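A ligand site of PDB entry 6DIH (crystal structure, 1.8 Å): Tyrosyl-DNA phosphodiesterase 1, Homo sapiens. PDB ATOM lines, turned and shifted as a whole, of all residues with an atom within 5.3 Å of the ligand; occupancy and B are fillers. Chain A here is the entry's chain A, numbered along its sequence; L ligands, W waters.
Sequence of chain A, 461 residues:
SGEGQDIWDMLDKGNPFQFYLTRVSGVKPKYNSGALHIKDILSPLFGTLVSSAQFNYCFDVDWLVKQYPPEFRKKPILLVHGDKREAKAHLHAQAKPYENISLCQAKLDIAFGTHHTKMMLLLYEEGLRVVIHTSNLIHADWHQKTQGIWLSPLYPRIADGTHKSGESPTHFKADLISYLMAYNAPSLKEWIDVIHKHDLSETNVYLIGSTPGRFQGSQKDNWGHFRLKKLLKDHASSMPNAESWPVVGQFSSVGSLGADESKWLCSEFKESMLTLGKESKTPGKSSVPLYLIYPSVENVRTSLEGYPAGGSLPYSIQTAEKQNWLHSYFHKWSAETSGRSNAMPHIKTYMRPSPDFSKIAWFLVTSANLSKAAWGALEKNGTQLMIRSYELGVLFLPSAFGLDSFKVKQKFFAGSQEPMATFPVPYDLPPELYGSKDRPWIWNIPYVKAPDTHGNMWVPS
The side-chain amino group (NZ) of Lys 118 lies within salt-bridge range of an oxygen (O2) of the ligand, 2.5 Å away. NZ of Lys 348 lies within salt-bridge range of O4 of the ligand, at 2.7 Å. O5 of the ligand is in hydrogen-bond range of OG of Ser 252, at 2.7 Å. NE2 of His 346 is in hydrogen-bond range of O1 of the ligand (2.7 Å). The side-chain amide nitrogen (ND2) of Asn 136 sits at hydrogen-bond distance from an oxygen (O1) of the ligand, 2.8 Å away. ND1 of His 116 lies within hydrogen-bond range of O2 of the ligand. The side-chain amide nitrogen (ND2) of Asn 369 lies within hydrogen-bond range of an oxygen (O4) of the ligand (3.1 Å).
The side-chain amino group (NZ) of Lys 118 is in hydrogen-bond range of the backbone carbonyl oxygen (O) of His 116. NZ of Lys 348 is in hydrogen-bond range of OG of Ser 252. The side-chain amino group (NZ) of Lys 348 lies within hydrogen-bond range of the backbone carbonyl oxygen (O) of His 346, 2.8 Å away. N of Ser 252 is in hydrogen-bond range of OD1 of Asn 369 (2.9 Å). ND2 of Asn 136 sits close to NE2 of His 346 (3.5 Å). The backbone NH of Asn 136 sits at hydrogen-bond distance from the side-chain carboxylate of Asp 141 (2.8 Å). The side-chain amide oxygen (OD1) of Asn 369 lies within hydrogen-bond range of the backbone NH (N) of Ser 253 (3.2 Å). The backbone carbonyl oxygen (O) of Pro 314 is in hydrogen-bond range of the side-chain hydroxyl (OG) of Ser 253, 3.5 Å away.
Water W1 lies within hydrogen-bond range of the side-chain hydroxyl of Ser 253 (2.5 Å) and an oxygen (O3) of the ligand (2.6 Å).
CB of Tyr 57 touches O2 of the ligand, at 3.5 Å. CG of Pro 314 touches C7 of the ligand (3.5 Å). Hydrophobic or aromatic side chains that line the ligand: Tyr 57, His 116, Pro 314 and His 346. Nine residues have an atom within 4 Å of the ligand: Tyr 57, His 116, Lys 118, Asn 136, Ser 252, Pro 314, His 346, Lys 348 and Asn 369.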
ATOM      1  N   TYR A  57      13.220   6.865  21.647  1.00  0.00           N
ATOM      2  CA  TYR A  57      13.251   8.117  22.389  1.00  0.00           C
ATOM      3  C   TYR A  57      11.891   8.411  23.010  1.00  0.00           C
ATOM      4  O   TYR A  57      11.774   8.592  24.224  1.00  0.00           O
ATOM      5  CB  TYR A  57      13.681   9.261  21.468  1.00  0.00           C
ATOM      6  CG  TYR A  57      13.487  10.604  22.134  1.00  0.00           C
ATOM      7  CD1 TYR A  57      14.343  11.028  23.146  1.00  0.00           C
ATOM      8  CD2 TYR A  57      12.421  11.426  21.779  1.00  0.00           C
ATOM      9  CE1 TYR A  57      14.150  12.251  23.774  1.00  0.00           C
ATOM     10  CE2 TYR A  57      12.232  12.640  22.393  1.00  0.00           C
ATOM     11  CZ  TYR A  57      13.088  13.047  23.387  1.00  0.00           C
ATOM     12  OH  TYR A  57      12.864  14.263  23.988  1.00  0.00           O
ATOM     13  N   HIS A 116      18.683   8.371  21.851  1.00  0.00           N
ATOM     14  CA  HIS A 116      18.117   8.573  20.509  1.00  0.00           C
ATOM     15  C   HIS A 116      17.993   7.291  19.705  1.00  0.00           C
ATOM     16  O   HIS A 116      17.199   7.250  18.757  1.00  0.00           O
ATOM     17  CB  HIS A 116      18.999   9.512  19.676  1.00  0.00           C
ATOM     18  CG  HIS A 116      18.739  10.963  19.884  1.00  0.00           C
ATOM     19  ND1 HIS A 116      17.506  11.540  19.655  1.00  0.00           N
ATOM     20  CD2 HIS A 116      19.576  11.973  20.225  1.00  0.00           C
ATOM     21  CE1 HIS A 116      17.582  12.839  19.900  1.00  0.00           C
ATOM     22  NE2 HIS A 116      18.825  13.121  20.252  1.00  0.00           N
ATOM     23  N   LYS A 118      17.059   4.084  17.798  1.00  0.00           N
ATOM     24  CA  LYS A 118      15.787   3.471  17.417  1.00  0.00           C
ATOM     25  C   LYS A 118      16.056   2.098  16.830  1.00  0.00           C
ATOM     26  O   LYS A 118      16.649   1.965  15.745  1.00  0.00           O
ATOM     27  CB  LYS A 118      15.027   4.390  16.473  1.00  0.00           C
ATOM     28  CG  LYS A 118      14.661   5.663  17.217  1.00  0.00           C
ATOM     29  CD  LYS A 118      14.259   6.764  16.286  1.00  0.00           C
ATOM     30  CE  LYS A 118      13.913   8.024  17.059  1.00  0.00           C
ATOM     31  NZ  LYS A 118      15.110   8.693  17.578  1.00  0.00           N
ATOM     32  N   ASN A 136      10.246   7.435  15.904  1.00  0.00           N
ATOM     33  CA  ASN A 136       9.702   7.283  17.255  1.00  0.00           C
ATOM     34  C   ASN A 136       8.478   6.380  17.235  1.00  0.00           C
ATOM     35  O   ASN A 136       7.859   6.156  16.191  1.00  0.00           O
ATOM     36  CB  ASN A 136       9.347   8.644  17.842  1.00  0.00           C
ATOM     37  CG  ASN A 136      10.572   9.473  18.135  1.00  0.00           C
ATOM     38  OD1 ASN A 136      11.229   9.273  19.160  1.00  0.00           O
ATOM     39  ND2 ASN A 136      10.914  10.401  17.229  1.00  0.00           N
ATOM     40  N   ASP A 141       4.980   9.698  13.694  1.00  0.00           N
ATOM     41  CA  ASP A 141       6.253   9.420  13.041  1.00  0.00           C
ATOM     42  C   ASP A 141       6.131   8.407  11.914  1.00  0.00           C
ATOM     43  O   ASP A 141       7.075   8.301  11.113  1.00  0.00           O
ATOM     44  CB  ASP A 141       7.287   8.943  14.054  1.00  0.00           C
ATOM     45  CG  ASP A 141       8.159  10.087  14.549  1.00  0.00           C
ATOM     46  OD1 ASP A 141       7.632  11.207  14.733  1.00  0.00           O
ATOM     47  OD2 ASP A 141       9.374   9.854  14.755  1.00  0.00           O
ATOM     48  N   SER A 252      17.405  15.901  10.747  1.00  0.00           N
ATOM     49  CA  SER A 252      16.184  16.575  11.198  1.00  0.00           C
ATOM     50  C   SER A 252      16.415  17.551  12.349  1.00  0.00           C
ATOM     51  O   SER A 252      15.472  18.214  12.793  1.00  0.00           O
ATOM     52  CB  SER A 252      15.135  15.538  11.610  1.00  0.00           C
ATOM     53  OG  SER A 252      15.580  14.742  12.690  1.00  0.00           O
ATOM     54  N   SER A 253      17.650  17.694  12.828  1.00  0.00           N
ATOM     55  CA  SER A 253      17.920  18.552  13.967  1.00  0.00           C
ATOM     56  C   SER A 253      19.380  18.994  13.902  1.00  0.00           C
ATOM     57  O   SER A 253      20.220  18.296  13.339  1.00  0.00           O
ATOM     58  CB  SER A 253      17.640  17.826  15.285  1.00  0.00           C
ATOM     59  OG  SER A 253      17.636  18.714  16.384  1.00  0.00           O
ATOM     60  N   SER A 312       8.754  18.227  14.802  1.00  0.00           N
ATOM     61  CA  SER A 312       9.719  17.128  14.744  1.00  0.00           C
ATOM     62  C   SER A 312      11.023  17.530  14.057  1.00  0.00           C
ATOM     63  O   SER A 312      11.795  16.667  13.616  1.00  0.00           O
ATOM     64  CB  SER A 312       9.106  15.932  14.028  1.00  0.00           C
ATOM     65  OG  SER A 312       7.993  15.451  14.750  1.00  0.00           O
ATOM     66  N   PRO A 314      13.553  20.003  15.492  1.00  0.00           N
ATOM     67  CA  PRO A 314      13.743  20.895  16.660  1.00  0.00           C
ATOM     68  C   PRO A 314      15.033  21.708  16.682  1.00  0.00           C
ATOM     69  O   PRO A 314      15.916  21.533  17.526  1.00  0.00           O
ATOM     70  CB  PRO A 314      13.667  19.904  17.830  1.00  0.00           C
ATOM     71  CG  PRO A 314      14.163  18.630  17.279  1.00  0.00           C
ATOM     72  CD  PRO A 314      13.802  18.584  15.806  1.00  0.00           C
ATOM     73  N   HIS A 346      12.382  12.697   8.851  1.00  0.00           N
ATOM     74  CA  HIS A 346      12.921  12.386  10.168  1.00  0.00           C
ATOM     75  C   HIS A 346      14.028  11.325  10.092  1.00  0.00           C
ATOM     76  O   HIS A 346      14.692  11.055  11.099  1.00  0.00           O
ATOM     77  CB  HIS A 346      11.781  11.925  11.102  1.00  0.00           C
ATOM     78  CG  HIS A 346      12.176  11.805  12.542  1.00  0.00           C
ATOM     79  ND1 HIS A 346      12.535  10.593  13.111  1.00  0.00           N
ATOM     80  CD2 HIS A 346      12.236  12.712  13.545  1.00  0.00           C
ATOM     81  CE1 HIS A 346      12.815  10.777  14.385  1.00  0.00           C
ATOM     82  NE2 HIS A 346      12.645  12.050  14.678  1.00  0.00           N
ATOM     83  N   LYS A 348      17.811  10.227   9.071  1.00  0.00           N
ATOM     84  CA  LYS A 348      19.103  10.897   8.991  1.00  0.00           C
ATOM     85  C   LYS A 348      20.008  10.039   8.118  1.00  0.00           C
ATOM     86  O   LYS A 348      20.063   8.823   8.317  1.00  0.00           O
ATOM     87  CB  LYS A 348      19.765  11.113  10.359  1.00  0.00           C
ATOM     88  CG  LYS A 348      18.938  11.938  11.343  1.00  0.00           C
ATOM     89  CD  LYS A 348      18.004  11.058  12.142  1.00  0.00           C
ATOM     90  CE  LYS A 348      17.461  11.850  13.326  1.00  0.00           C
ATOM     91  NZ  LYS A 348      16.007  11.697  13.488  1.00  0.00           N
ATOM     92  N   SER A 367      20.321   7.294  13.512  1.00  0.00           N
ATOM     93  CA  SER A 367      19.588   8.232  14.344  1.00  0.00           C
ATOM     94  C   SER A 367      20.332   9.530  14.579  1.00  0.00           C
ATOM     95  O   SER A 367      19.734  10.496  15.063  1.00  0.00           O
ATOM     96  CB  SER A 367      19.274   7.582  15.701  1.00  0.00           C
ATOM     97  OG  SER A 367      20.493   7.228  16.366  1.00  0.00           O
ATOM     98  N   ASN A 369      21.776  13.058  14.444  1.00  0.00           N
ATOM     99  CA  ASN A 369      21.608  14.369  13.821  1.00  0.00           C
ATOM    100  C   ASN A 369      22.941  15.103  13.715  1.00  0.00           C
ATOM    101  O   ASN A 369      23.996  14.568  14.057  1.00  0.00           O
ATOM    102  CB  ASN A 369      20.579  15.183  14.624  1.00  0.00           C
ATOM    103  CG  ASN A 369      19.167  14.828  14.240  1.00  0.00           C
ATOM    104  OD1 ASN A 369      18.832  14.772  13.058  1.00  0.00           O
ATOM    105  ND2 ASN A 369      18.325  14.550  15.237  1.00  0.00           N
HETATM  106  C1  LIG L   1      15.206  14.295  17.711  1.00  0.00           C
HETATM  107  C2  LIG L   1      14.227  11.995  18.131  1.00  0.00           C
HETATM  108  C3  LIG L   1      14.703  13.367  18.606  1.00  0.00           C
HETATM  109  C4  LIG L   1      14.604  13.674  19.959  1.00  0.00           C
HETATM  110  C5  LIG L   1      15.029  14.910  20.418  1.00  0.00           C
HETATM  111  C6  LIG L   1      15.546  15.842  19.525  1.00  0.00           C
HETATM  112  C7  LIG L   1      15.636  15.538  18.173  1.00  0.00           C
HETATM  113  C8  LIG L   1      15.321  13.970  16.211  1.00  0.00           C
HETATM  114  O1  LIG L   1      13.294  11.895  17.301  1.00  0.00           O
HETATM  115  O2  LIG L   1      14.768  10.966  18.582  1.00  0.00           O
HETATM  116  O3  LIG L   1      15.981  17.097  19.982  1.00  0.00           O
HETATM  117  O4  LIG L   1      15.803  12.875  15.861  1.00  0.00           O
HETATM  118  O5  LIG L   1      14.962  14.792  15.320  1.00  0.00           O
HETATM  119  O   HOH W   1      17.902  18.489  18.887  1.00  0.00           O
